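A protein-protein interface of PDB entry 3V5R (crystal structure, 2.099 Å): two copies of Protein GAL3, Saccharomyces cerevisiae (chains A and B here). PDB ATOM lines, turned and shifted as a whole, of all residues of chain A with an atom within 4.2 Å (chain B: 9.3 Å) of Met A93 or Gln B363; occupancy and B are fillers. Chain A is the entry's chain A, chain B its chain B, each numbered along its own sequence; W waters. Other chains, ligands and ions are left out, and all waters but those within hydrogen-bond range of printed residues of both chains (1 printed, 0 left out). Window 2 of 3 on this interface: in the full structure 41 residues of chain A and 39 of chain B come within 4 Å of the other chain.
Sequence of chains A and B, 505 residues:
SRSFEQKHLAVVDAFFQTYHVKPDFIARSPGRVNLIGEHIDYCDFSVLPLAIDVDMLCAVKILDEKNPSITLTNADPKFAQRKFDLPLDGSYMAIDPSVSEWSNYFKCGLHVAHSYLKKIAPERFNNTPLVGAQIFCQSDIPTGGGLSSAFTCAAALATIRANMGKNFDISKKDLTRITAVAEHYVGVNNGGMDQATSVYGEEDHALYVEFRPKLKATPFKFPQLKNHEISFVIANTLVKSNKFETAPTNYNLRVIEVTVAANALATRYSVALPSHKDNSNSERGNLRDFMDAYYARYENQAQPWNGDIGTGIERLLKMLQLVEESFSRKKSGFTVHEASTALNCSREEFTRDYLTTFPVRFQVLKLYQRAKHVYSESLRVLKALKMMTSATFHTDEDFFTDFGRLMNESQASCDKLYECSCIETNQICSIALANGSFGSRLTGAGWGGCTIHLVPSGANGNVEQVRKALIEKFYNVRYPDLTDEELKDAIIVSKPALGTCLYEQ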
ATOM      1  N   PHE A  84      19.014 -16.363  -6.754  1.00  0.00           N
ATOM      2  CA  PHE A  84      18.454 -17.189  -7.818  1.00  0.00           C
ATOM      3  C   PHE A  84      18.383 -16.444  -9.142  1.00  0.00           C
ATOM      4  O   PHE A  84      18.213 -15.226  -9.178  1.00  0.00           O
ATOM      5  CB  PHE A  84      17.074 -17.723  -7.434  1.00  0.00           C
ATOM      6  CG  PHE A  84      16.159 -16.682  -6.868  1.00  0.00           C
ATOM      7  CD1 PHE A  84      15.374 -15.910  -7.700  1.00  0.00           C
ATOM      8  CD2 PHE A  84      16.086 -16.479  -5.498  1.00  0.00           C
ATOM      9  CE1 PHE A  84      14.531 -14.951  -7.178  1.00  0.00           C
ATOM     10  CE2 PHE A  84      15.256 -15.528  -4.970  1.00  0.00           C
ATOM     11  CZ  PHE A  84      14.477 -14.758  -5.806  1.00  0.00           C
ATOM     12  N   ASP A  85      18.531 -17.195 -10.224  1.00  0.00           N
ATOM     13  CA  ASP A  85      18.504 -16.636 -11.563  1.00  0.00           C
ATOM     14  C   ASP A  85      17.070 -16.598 -12.070  1.00  0.00           C
ATOM     15  O   ASP A  85      16.325 -17.564 -11.915  1.00  0.00           O
ATOM     16  CB  ASP A  85      19.361 -17.485 -12.504  1.00  0.00           C
ATOM     17  CG  ASP A  85      20.845 -17.375 -12.206  1.00  0.00           C
ATOM     18  OD1 ASP A  85      21.283 -16.318 -11.701  1.00  0.00           O
ATOM     19  OD2 ASP A  85      21.578 -18.346 -12.486  1.00  0.00           O
ATOM     20  N   PRO A  87      14.318 -16.919 -14.897  1.00  0.00           N
ATOM     21  CA  PRO A  87      14.295 -17.711 -16.134  1.00  0.00           C
ATOM     22  C   PRO A  87      14.437 -16.828 -17.378  1.00  0.00           C
ATOM     23  O   PRO A  87      13.719 -15.835 -17.514  1.00  0.00           O
ATOM     24  CB  PRO A  87      12.910 -18.365 -16.108  1.00  0.00           C
ATOM     25  CG  PRO A  87      12.518 -18.372 -14.666  1.00  0.00           C
ATOM     26  CD  PRO A  87      13.090 -17.091 -14.110  1.00  0.00           C
ATOM     27  N   SER A  91       9.552 -17.173 -18.170  1.00  0.00           N
ATOM     28  CA  SER A  91       8.573 -17.979 -17.461  1.00  0.00           C
ATOM     29  C   SER A  91       8.603 -17.642 -15.986  1.00  0.00           C
ATOM     30  O   SER A  91       9.586 -17.103 -15.482  1.00  0.00           O
ATOM     31  CB  SER A  91       8.842 -19.476 -17.667  1.00  0.00           C
ATOM     32  OG  SER A  91      10.084 -19.860 -17.102  1.00  0.00           O
ATOM     33  N   TYR A  92       7.520 -17.957 -15.288  1.00  0.00           N
ATOM     34  CA  TYR A  92       7.473 -17.725 -13.857  1.00  0.00           C
ATOM     35  C   TYR A  92       8.510 -18.576 -13.145  1.00  0.00           C
ATOM     36  O   TYR A  92       8.706 -19.741 -13.485  1.00  0.00           O
ATOM     37  CB  TYR A  92       6.085 -18.039 -13.306  1.00  0.00           C
ATOM     38  CG  TYR A  92       4.982 -17.207 -13.915  1.00  0.00           C
ATOM     39  CD1 TYR A  92       4.957 -15.822 -13.759  1.00  0.00           C
ATOM     40  CD2 TYR A  92       3.954 -17.809 -14.629  1.00  0.00           C
ATOM     41  CE1 TYR A  92       3.940 -15.065 -14.310  1.00  0.00           C
ATOM     42  CE2 TYR A  92       2.935 -17.063 -15.179  1.00  0.00           C
ATOM     43  CZ  TYR A  92       2.931 -15.691 -15.017  1.00  0.00           C
ATOM     44  OH  TYR A  92       1.907 -14.962 -15.572  1.00  0.00           O
ATOM     45  N   MET A  93       9.187 -17.966 -12.174  1.00  0.00           N
ATOM     46  CA  MET A  93      10.045 -18.679 -11.237  1.00  0.00           C
ATOM     47  C   MET A  93       9.311 -19.884 -10.684  1.00  0.00           C
ATOM     48  O   MET A  93       8.093 -19.857 -10.511  1.00  0.00           O
ATOM     49  CB  MET A  93      10.393 -17.770 -10.055  1.00  0.00           C
ATOM     50  CG  MET A  93      11.553 -16.828 -10.272  1.00  0.00           C
ATOM     51  SD  MET A  93      13.102 -17.698 -10.042  1.00  0.00           S
ATOM     52  CE  MET A  93      12.834 -18.412  -8.422  1.00  0.00           C
ATOM     53  N   ALA A  94      10.053 -20.941 -10.390  1.00  0.00           N
ATOM     54  CA  ALA A  94       9.469 -22.091  -9.729  1.00  0.00           C
ATOM     55  C   ALA A  94       9.397 -21.842  -8.228  1.00  0.00           C
ATOM     56  O   ALA A  94      10.398 -21.510  -7.591  1.00  0.00           O
ATOM     57  CB  ALA A  94      10.284 -23.350 -10.028  1.00  0.00           C
ATOM     58  N   ILE A  95       8.202 -21.970  -7.672  1.00  0.00           N
ATOM     59  CA  ILE A  95       7.997 -21.887  -6.230  1.00  0.00           C
ATOM     60  C   ILE A  95       7.408 -23.211  -5.751  1.00  0.00           C
ATOM     61  O   ILE A  95       6.504 -23.757  -6.387  1.00  0.00           O
ATOM     62  CB  ILE A  95       7.005 -20.756  -5.866  1.00  0.00           C
ATOM     63  CG1 ILE A  95       7.438 -19.415  -6.481  1.00  0.00           C
ATOM     64  CG2 ILE A  95       6.839 -20.642  -4.351  1.00  0.00           C
ATOM     65  CD1 ILE A  95       6.412 -18.295  -6.280  1.00  0.00           C
ATOM     66  N   LYS A 107       8.938 -14.502  -3.369  1.00  0.00           N
ATOM     67  CA  LYS A 107       8.697 -15.122  -4.661  1.00  0.00           C
ATOM     68  C   LYS A 107       7.234 -15.020  -5.084  1.00  0.00           C
ATOM     69  O   LYS A 107       6.958 -14.849  -6.263  1.00  0.00           O
ATOM     70  CB  LYS A 107       9.195 -16.562  -4.668  1.00  0.00           C
ATOM     71  CG  LYS A 107      10.712 -16.651  -4.489  1.00  0.00           C
ATOM     72  CD  LYS A 107      11.221 -18.043  -4.806  1.00  0.00           C
ATOM     73  CE  LYS A 107      12.740 -18.111  -4.739  1.00  0.00           C
ATOM     74  NZ  LYS A 107      13.210 -19.490  -5.051  1.00  0.00           N
ATOM     75  N   LEU A 110       6.889 -11.468  -6.311  1.00  0.00           N
ATOM     76  CA  LEU A 110       7.542 -11.381  -7.611  1.00  0.00           C
ATOM     77  C   LEU A 110       6.652 -11.980  -8.689  1.00  0.00           C
ATOM     78  O   LEU A 110       6.522 -11.434  -9.782  1.00  0.00           O
ATOM     79  CB  LEU A 110       8.874 -12.124  -7.569  1.00  0.00           C
ATOM     80  CG  LEU A 110       9.707 -12.251  -8.848  1.00  0.00           C
ATOM     81  CD1 LEU A 110      10.605 -11.066  -9.023  1.00  0.00           C
ATOM     82  CD2 LEU A 110      10.542 -13.521  -8.808  1.00  0.00           C
ATOM     83  N   HIS A 111       6.030 -13.107  -8.363  1.00  0.00           N
ATOM     84  CA  HIS A 111       5.179 -13.814  -9.302  1.00  0.00           C
ATOM     85  C   HIS A 111       3.939 -13.012  -9.693  1.00  0.00           C
ATOM     86  O   HIS A 111       3.606 -12.917 -10.876  1.00  0.00           O
ATOM     87  CB  HIS A 111       4.730 -15.164  -8.716  1.00  0.00           C
ATOM     88  CG  HIS A 111       3.898 -15.978  -9.659  1.00  0.00           C
ATOM     89  ND1 HIS A 111       4.373 -17.108 -10.283  1.00  0.00           N
ATOM     90  CD2 HIS A 111       2.626 -15.816 -10.094  1.00  0.00           C
ATOM     91  CE1 HIS A 111       3.429 -17.614 -11.058  1.00  0.00           C
ATOM     92  NE2 HIS A 111       2.358 -16.846 -10.964  1.00  0.00           N
ATOM     93  N   TYR A 185      -0.694 -19.402  -2.640  1.00  0.00           N
ATOM     94  CA  TYR A 185       0.727 -19.752  -2.564  1.00  0.00           C
ATOM     95  C   TYR A 185       1.126 -19.913  -1.110  1.00  0.00           C
ATOM     96  O   TYR A 185       2.067 -20.648  -0.775  1.00  0.00           O
ATOM     97  CB  TYR A 185       1.601 -18.653  -3.172  1.00  0.00           C
ATOM     98  CG  TYR A 185       1.609 -18.606  -4.678  1.00  0.00           C
ATOM     99  CD1 TYR A 185       2.415 -19.465  -5.414  1.00  0.00           C
ATOM    100  CD2 TYR A 185       0.824 -17.694  -5.361  1.00  0.00           C
ATOM    101  CE1 TYR A 185       2.426 -19.418  -6.797  1.00  0.00           C
ATOM    102  CE2 TYR A 185       0.825 -17.638  -6.734  1.00  0.00           C
ATOM    103  CZ  TYR A 185       1.624 -18.501  -7.449  1.00  0.00           C
ATOM    104  OH  TYR A 185       1.619 -18.436  -8.821  1.00  0.00           O
ATOM    105  N   PRO B 248      -2.124 -28.074   3.719  1.00  0.00           N
ATOM    106  CA  PRO B 248      -2.590 -27.318   2.561  1.00  0.00           C
ATOM    107  C   PRO B 248      -1.909 -27.793   1.292  1.00  0.00           C
ATOM    108  O   PRO B 248      -2.406 -27.512   0.211  1.00  0.00           O
ATOM    109  CB  PRO B 248      -2.146 -25.878   2.881  1.00  0.00           C
ATOM    110  CG  PRO B 248      -1.893 -25.858   4.350  1.00  0.00           C
ATOM    111  CD  PRO B 248      -1.373 -27.225   4.658  1.00  0.00           C
ATOM    112  N   THR B 249      -0.781 -28.486   1.405  1.00  0.00           N
ATOM    113  CA  THR B 249      -0.166 -29.056   0.208  1.00  0.00           C
ATOM    114  C   THR B 249      -0.565 -30.517  -0.015  1.00  0.00           C
ATOM    115  O   THR B 249      -0.254 -31.092  -1.065  1.00  0.00           O
ATOM    116  CB  THR B 249       1.380 -28.962   0.229  1.00  0.00           C
ATOM    117  OG1 THR B 249       1.895 -29.749   1.309  1.00  0.00           O
ATOM    118  CG2 THR B 249       1.832 -27.530   0.394  1.00  0.00           C
ATOM    119  N   LEU B 253      -5.324 -30.111  -0.954  1.00  0.00           N
ATOM    120  CA  LEU B 253      -4.966 -29.829  -2.330  1.00  0.00           C
ATOM    121  C   LEU B 253      -5.501 -30.942  -3.232  1.00  0.00           C
ATOM    122  O   LEU B 253      -5.979 -30.671  -4.334  1.00  0.00           O
ATOM    123  CB  LEU B 253      -3.449 -29.678  -2.465  1.00  0.00           C
ATOM    124  CG  LEU B 253      -2.851 -29.456  -3.854  1.00  0.00           C
ATOM    125  CD1 LEU B 253      -3.556 -28.316  -4.561  1.00  0.00           C
ATOM    126  CD2 LEU B 253      -1.349 -29.182  -3.748  1.00  0.00           C
ATOM    127  N   GLU B 257      -7.823 -30.638  -6.410  1.00  0.00           N
ATOM    128  CA  GLU B 257      -7.360 -31.129  -7.702  1.00  0.00           C
ATOM    129  C   GLU B 257      -8.335 -32.109  -8.375  1.00  0.00           C
ATOM    130  O   GLU B 257      -8.605 -31.988  -9.574  1.00  0.00           O
ATOM    131  CB  GLU B 257      -5.958 -31.730  -7.583  1.00  0.00           C
ATOM    132  CG  GLU B 257      -4.856 -30.678  -7.352  1.00  0.00           C
ATOM    133  CD  GLU B 257      -3.507 -31.315  -7.059  1.00  0.00           C
ATOM    134  OE1 GLU B 257      -3.447 -32.229  -6.204  1.00  0.00           O
ATOM    135  OE2 GLU B 257      -2.510 -30.918  -7.699  1.00  0.00           O
ATOM    136  N   SER B 332       2.705 -30.348 -16.811  1.00  0.00           N
ATOM    137  CA  SER B 332       3.259 -29.248 -16.020  1.00  0.00           C
ATOM    138  C   SER B 332       2.294 -28.783 -14.924  1.00  0.00           C
ATOM    139  O   SER B 332       2.715 -28.174 -13.941  1.00  0.00           O
ATOM    140  CB  SER B 332       3.602 -28.053 -16.922  1.00  0.00           C
ATOM    141  OG  SER B 332       4.454 -28.430 -17.990  1.00  0.00           O
ATOM    142  N   GLY B 333       1.002 -29.067 -15.102  1.00  0.00           N
ATOM    143  CA  GLY B 333      -0.012 -28.650 -14.150  1.00  0.00           C
ATOM    144  C   GLY B 333      -0.645 -27.337 -14.569  1.00  0.00           C
ATOM    145  O   GLY B 333      -0.119 -26.636 -15.437  1.00  0.00           O
ATOM    146  N   PHE B 334      -1.775 -27.003 -13.953  1.00  0.00           N
ATOM    147  CA  PHE B 334      -2.527 -25.798 -14.314  1.00  0.00           C
ATOM    148  C   PHE B 334      -2.350 -24.719 -13.264  1.00  0.00           C
ATOM    149  O   PHE B 334      -2.546 -24.977 -12.077  1.00  0.00           O
ATOM    150  CB  PHE B 334      -4.032 -26.101 -14.433  1.00  0.00           C
ATOM    151  CG  PHE B 334      -4.386 -27.019 -15.569  1.00  0.00           C
ATOM    152  CD1 PHE B 334      -3.965 -28.337 -15.572  1.00  0.00           C
ATOM    153  CD2 PHE B 334      -5.160 -26.567 -16.625  1.00  0.00           C
ATOM    154  CE1 PHE B 334      -4.297 -29.191 -16.620  1.00  0.00           C
ATOM    155  CE2 PHE B 334      -5.492 -27.409 -17.672  1.00  0.00           C
ATOM    156  CZ  PHE B 334      -5.055 -28.729 -17.666  1.00  0.00           C
ATOM    157  N   THR B 335      -1.989 -23.512 -13.697  1.00  0.00           N
ATOM    158  CA  THR B 335      -2.100 -22.333 -12.843  1.00  0.00           C
ATOM    159  C   THR B 335      -3.583 -22.054 -12.587  1.00  0.00           C
ATOM    160  O   THR B 335      -4.456 -22.629 -13.241  1.00  0.00           O
ATOM    161  CB  THR B 335      -1.516 -21.069 -13.514  1.00  0.00           C
ATOM    162  OG1 THR B 335      -2.181 -20.843 -14.766  1.00  0.00           O
ATOM    163  CG2 THR B 335      -0.004 -21.206 -13.741  1.00  0.00           C
ATOM    164  N   VAL B 336      -3.866 -21.169 -11.640  1.00  0.00           N
ATOM    165  CA  VAL B 336      -5.241 -20.768 -11.401  1.00  0.00           C
ATOM    166  C   VAL B 336      -5.839 -20.185 -12.675  1.00  0.00           C
ATOM    167  O   VAL B 336      -6.971 -20.493 -13.033  1.00  0.00           O
ATOM    168  CB  VAL B 336      -5.348 -19.745 -10.266  1.00  0.00           C
ATOM    169  CG1 VAL B 336      -6.777 -19.196 -10.195  1.00  0.00           C
ATOM    170  CG2 VAL B 336      -4.949 -20.405  -8.947  1.00  0.00           C
ATOM    171  N   HIS B 337      -5.062 -19.360 -13.373  1.00  0.00           N
ATOM    172  CA  HIS B 337      -5.539 -18.750 -14.610  1.00  0.00           C
ATOM    173  C   HIS B 337      -5.894 -19.828 -15.639  1.00  0.00           C
ATOM    174  O   HIS B 337      -6.968 -19.794 -16.243  1.00  0.00           O
ATOM    175  CB  HIS B 337      -4.499 -17.771 -15.176  1.00  0.00           C
ATOM    176  CG  HIS B 337      -5.081 -16.730 -16.079  1.00  0.00           C
ATOM    177  ND1 HIS B 337      -6.182 -16.965 -16.874  1.00  0.00           N
ATOM    178  CD2 HIS B 337      -4.725 -15.442 -16.301  1.00  0.00           C
ATOM    179  CE1 HIS B 337      -6.473 -15.871 -17.555  1.00  0.00           C
ATOM    180  NE2 HIS B 337      -5.606 -14.932 -17.223  1.00  0.00           N
ATOM    181  N   GLU B 338      -5.001 -20.797 -15.814  1.00  0.00           N
ATOM    182  CA  GLU B 338      -5.235 -21.885 -16.758  1.00  0.00           C
ATOM    183  C   GLU B 338      -6.410 -22.766 -16.347  1.00  0.00           C
ATOM    184  O   GLU B 338      -7.153 -23.267 -17.197  1.00  0.00           O
ATOM    185  CB  GLU B 338      -3.973 -22.731 -16.916  1.00  0.00           C
ATOM    186  CG  GLU B 338      -2.901 -22.058 -17.768  1.00  0.00           C
ATOM    187  CD  GLU B 338      -1.518 -22.622 -17.502  1.00  0.00           C
ATOM    188  OE1 GLU B 338      -1.358 -23.387 -16.524  1.00  0.00           O
ATOM    189  OE2 GLU B 338      -0.589 -22.295 -18.270  1.00  0.00           O
ATOM    190  N   ALA B 339      -6.571 -22.961 -15.042  1.00  0.00           N
ATOM    191  CA  ALA B 339      -7.673 -23.762 -14.534  1.00  0.00           C
ATOM    192  C   ALA B 339      -9.006 -23.061 -14.814  1.00  0.00           C
ATOM    193  O   ALA B 339      -9.970 -23.704 -15.230  1.00  0.00           O
ATOM    194  CB  ALA B 339      -7.497 -24.030 -13.042  1.00  0.00           C
ATOM    195  N   ARG B 347     -11.389 -15.950 -13.154  1.00  0.00           N
ATOM    196  CA  ARG B 347     -10.575 -16.243 -11.994  1.00  0.00           C
ATOM    197  C   ARG B 347     -11.365 -16.060 -10.703  1.00  0.00           C
ATOM    198  O   ARG B 347     -11.233 -16.855  -9.782  1.00  0.00           O
ATOM    199  CB  ARG B 347      -9.342 -15.348 -11.965  1.00  0.00           C
ATOM    200  CG  ARG B 347      -8.367 -15.757 -10.880  1.00  0.00           C
ATOM    201  CD  ARG B 347      -7.152 -14.859 -10.799  1.00  0.00           C
ATOM    202  NE  ARG B 347      -6.023 -15.578 -10.214  1.00  0.00           N
ATOM    203  CZ  ARG B 347      -4.975 -16.008 -10.910  1.00  0.00           C
ATOM    204  NH1 ARG B 347      -4.895 -15.781 -12.213  1.00  0.00           N
ATOM    205  NH2 ARG B 347      -3.996 -16.656 -10.303  1.00  0.00           N
ATOM    206  N   PHE B 350     -13.619 -18.992 -10.365  1.00  0.00           N
ATOM    207  CA  PHE B 350     -12.835 -20.179 -10.046  1.00  0.00           C
ATOM    208  C   PHE B 350     -12.432 -20.164  -8.572  1.00  0.00           C
ATOM    209  O   PHE B 350     -12.565 -21.169  -7.868  1.00  0.00           O
ATOM    210  CB  PHE B 350     -11.592 -20.304 -10.922  1.00  0.00           C
ATOM    211  CG  PHE B 350     -10.776 -21.534 -10.618  1.00  0.00           C
ATOM    212  CD1 PHE B 350     -11.088 -22.746 -11.208  1.00  0.00           C
ATOM    213  CD2 PHE B 350      -9.725 -21.489  -9.705  1.00  0.00           C
ATOM    214  CE1 PHE B 350     -10.359 -23.887 -10.918  1.00  0.00           C
ATOM    215  CE2 PHE B 350      -8.990 -22.634  -9.407  1.00  0.00           C
ATOM    216  CZ  PHE B 350      -9.311 -23.831 -10.010  1.00  0.00           C
ATOM    217  N   LEU B 355     -11.550 -22.487  -4.237  1.00  0.00           N
ATOM    218  CA  LEU B 355     -10.430 -22.127  -3.363  1.00  0.00           C
ATOM    219  C   LEU B 355     -10.843 -21.415  -2.066  1.00  0.00           C
ATOM    220  O   LEU B 355     -10.006 -20.802  -1.403  1.00  0.00           O
ATOM    221  CB  LEU B 355      -9.463 -21.211  -4.131  1.00  0.00           C
ATOM    222  CG  LEU B 355      -8.904 -21.724  -5.457  1.00  0.00           C
ATOM    223  CD1 LEU B 355      -7.919 -20.703  -6.030  1.00  0.00           C
ATOM    224  CD2 LEU B 355      -8.231 -23.065  -5.247  1.00  0.00           C
ATOM    225  N   VAL B 360      -5.071 -23.915   1.050  1.00  0.00           N
ATOM    226  CA  VAL B 360      -4.263 -24.694   0.120  1.00  0.00           C
ATOM    227  C   VAL B 360      -2.988 -23.971  -0.294  1.00  0.00           C
ATOM    228  O   VAL B 360      -2.929 -22.743  -0.314  1.00  0.00           O
ATOM    229  CB  VAL B 360      -5.060 -25.106  -1.141  1.00  0.00           C
ATOM    230  CG1 VAL B 360      -5.789 -26.409  -0.900  1.00  0.00           C
ATOM    231  CG2 VAL B 360      -6.017 -23.996  -1.574  1.00  0.00           C
ATOM    232  N   ARG B 361      -1.966 -24.744  -0.628  1.00  0.00           N
ATOM    233  CA  ARG B 361      -0.715 -24.189  -1.106  1.00  0.00           C
ATOM    234  C   ARG B 361      -0.311 -24.914  -2.369  1.00  0.00           C
ATOM    235  O   ARG B 361      -0.039 -26.114  -2.337  1.00  0.00           O
ATOM    236  CB  ARG B 361       0.392 -24.375  -0.071  1.00  0.00           C
ATOM    237  CG  ARG B 361       0.665 -23.175   0.800  1.00  0.00           C
ATOM    238  CD  ARG B 361       1.896 -23.353   1.697  1.00  0.00           C
ATOM    239  NE  ARG B 361       1.910 -24.647   2.370  1.00  0.00           N
ATOM    240  CZ  ARG B 361       2.852 -25.038   3.224  1.00  0.00           C
ATOM    241  NH1 ARG B 361       3.866 -24.227   3.508  1.00  0.00           N
ATOM    242  NH2 ARG B 361       2.786 -26.244   3.782  1.00  0.00           N
ATOM    243  N   PHE B 362      -0.254 -24.192  -3.480  1.00  0.00           N
ATOM    244  CA  PHE B 362       0.152 -24.805  -4.736  1.00  0.00           C
ATOM    245  C   PHE B 362       0.572 -23.716  -5.685  1.00  0.00           C
ATOM    246  O   PHE B 362       0.103 -22.590  -5.573  1.00  0.00           O
ATOM    247  CB  PHE B 362      -1.012 -25.595  -5.363  1.00  0.00           C
ATOM    248  CG  PHE B 362      -2.195 -24.742  -5.759  1.00  0.00           C
ATOM    249  CD1 PHE B 362      -2.344 -24.292  -7.069  1.00  0.00           C
ATOM    250  CD2 PHE B 362      -3.169 -24.406  -4.826  1.00  0.00           C
ATOM    251  CE1 PHE B 362      -3.436 -23.503  -7.435  1.00  0.00           C
ATOM    252  CE2 PHE B 362      -4.268 -23.626  -5.187  1.00  0.00           C
ATOM    253  CZ  PHE B 362      -4.401 -23.172  -6.494  1.00  0.00           C
ATOM    254  N   GLN B 363       1.447 -24.053  -6.623  1.00  0.00           N
ATOM    255  CA  GLN B 363       1.699 -23.162  -7.746  1.00  0.00           C
ATOM    256  C   GLN B 363       0.830 -23.637  -8.903  1.00  0.00           C
ATOM    257  O   GLN B 363       0.279 -22.832  -9.650  1.00  0.00           O
ATOM    258  CB  GLN B 363       3.184 -23.143  -8.137  1.00  0.00           C
ATOM    259  CG  GLN B 363       3.529 -22.070  -9.176  1.00  0.00           C
ATOM    260  CD  GLN B 363       5.029 -21.911  -9.412  1.00  0.00           C
ATOM    261  OE1 GLN B 363       5.817 -22.816  -9.126  1.00  0.00           O
ATOM    262  NE2 GLN B 363       5.430 -20.748  -9.923  1.00  0.00           N
ATOM    263  N   VAL B 364       0.693 -24.952  -9.032  1.00  0.00           N
ATOM    264  CA  VAL B 364      -0.148 -25.520 -10.075  1.00  0.00           C
ATOM    265  C   VAL B 364      -1.046 -26.623  -9.530  1.00  0.00           C
ATOM    266  O   VAL B 364      -0.736 -27.248  -8.514  1.00  0.00           O
ATOM    267  CB  VAL B 364       0.682 -26.086 -11.249  1.00  0.00           C
ATOM    268  CG1 VAL B 364       1.461 -24.960 -11.963  1.00  0.00           C
ATOM    269  CG2 VAL B 364       1.624 -27.182 -10.766  1.00  0.00           C
ATOM    270  N   LEU B 365      -2.166 -26.842 -10.210  1.00  0.00           N
ATOM    271  CA  LEU B 365      -3.026 -27.979  -9.939  1.00  0.00           C
ATOM    272  C   LEU B 365      -2.717 -29.053 -10.966  1.00  0.00           C
ATOM    273  O   LEU B 365      -2.795 -28.802 -12.167  1.00  0.00           O
ATOM    274  CB  LEU B 365      -4.490 -27.570 -10.029  1.00  0.00           C
ATOM    275  CG  LEU B 365      -4.889 -26.406  -9.120  1.00  0.00           C
ATOM    276  CD1 LEU B 365      -6.248 -25.845  -9.524  1.00  0.00           C
ATOM    277  CD2 LEU B 365      -4.912 -26.848  -7.674  1.00  0.00           C
ATOM    278  N   LYS B 366      -2.364 -30.246 -10.491  1.00  0.00           N
ATOM    279  CA  LYS B 366      -1.902 -31.321 -11.368  1.00  0.00           C
ATOM    280  C   LYS B 366      -3.040 -32.245 -11.788  1.00  0.00           C
ATOM    281  O   LYS B 366      -3.125 -33.402 -11.353  1.00  0.00           O
ATOM    282  CB  LYS B 366      -0.772 -32.103 -10.690  1.00  0.00           C
ATOM    283  CG  LYS B 366       0.510 -31.263 -10.505  1.00  0.00           C
ATOM    284  CD  LYS B 366       1.564 -32.019  -9.686  1.00  0.00           C
ATOM    285  CE  LYS B 366       2.783 -31.126  -9.379  1.00  0.00           C
ATOM    286  NZ  LYS B 366       3.774 -31.861  -8.535  1.00  0.00           N
ATOM    287  N   ARG B 370      -3.489 -36.423 -11.091  1.00  0.00           N
ATOM    288  CA  ARG B 370      -4.453 -36.766 -10.054  1.00  0.00           C
ATOM    289  C   ARG B 370      -5.616 -37.556 -10.647  1.00  0.00           C
ATOM    290  O   ARG B 370      -6.056 -38.550 -10.080  1.00  0.00           O
ATOM    291  CB  ARG B 370      -4.966 -35.510  -9.356  1.00  0.00           C
ATOM    292  CG  ARG B 370      -4.205 -35.114  -8.080  1.00  0.00           C
ATOM    293  CD  ARG B 370      -2.679 -35.133  -8.216  1.00  0.00           C
ATOM    294  NE  ARG B 370      -2.077 -34.162  -7.302  1.00  0.00           N
ATOM    295  CZ  ARG B 370      -0.773 -34.011  -7.072  1.00  0.00           C
ATOM    296  NH1 ARG B 370       0.124 -34.790  -7.669  1.00  0.00           N
ATOM    297  NH2 ARG B 370      -0.369 -33.073  -6.225  1.00  0.00           N
HETATM  298  O   HOH W   1       1.064 -20.297 -10.285  1.00  0.00           O
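The backbone carbonyl oxygen (O) of Met A93 is in hydrogen-bond range of the side-chain amide nitrogen (NE2) of Gln B363, at 2.9 Å.
The side-chain amide oxygen (OE1) of Gln B363 lies within hydrogen-bond range of the backbone NH (N) of Ile A95, 2.9 Å away.
A ring nitrogen (NE2) of His A111 is in hydrogen-bond range of the side-chain hydroxyl (OH) of Tyr A185 (2.8 Å).
N of Arg B361 sits at hydrogen-bond distance from O of Pro B248 (2.9 Å).
Among the printed residues, pairs that only touch across the chains: Ala A94 with Gln B363 (3.8 Å), His A111 with Gln B363 (3.8 Å), Tyr A185 with Arg B361 (3.3 Å), Tyr A185 with Phe B362 (3.9 Å) and Tyr A185 with Gln B363 (3.7 Å).
Met A93 touches one residue of chain B.
Of chain B, only Gln B363 (3.8 Å) comes within 4 Å of Ala A94.
Printed residues of chain B within 4 Å of Ile A95: Gln B363.
Leu B253 touches none of the printed residues of chain A.
Ala B339 touches none of the printed residues of chain A.
Printed residues of chain A within 4 Å of Phe B362: Tyr A185.
The nearest residue of chain B that does not touch Met A93 is Val B364 (8.5 Å).
The nearest printed residue of chain A that does not touch Gln B363 is Tyr A92 (4.4 Å).
Along chain B the printed residues that touch a printed residue of chain A span positions 361 to 363.
Of the 12 printed residues of chain A, 5 touch a printed residue of chain B.
Printed residues of chain A that touch a printed residue of chain B: Met A93, Ala A94, Ile A95, His A111 and Tyr A185.
No position is printed for both chains.
Of the 7 pairs that touch across the chains among the printed residues, none has its exchanged pair printed and touching as well.
Water W1 bridges the side-chain hydroxyl (OH) of Tyr A185 and the backbone carbonyl oxygen (O) of Gln B363.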
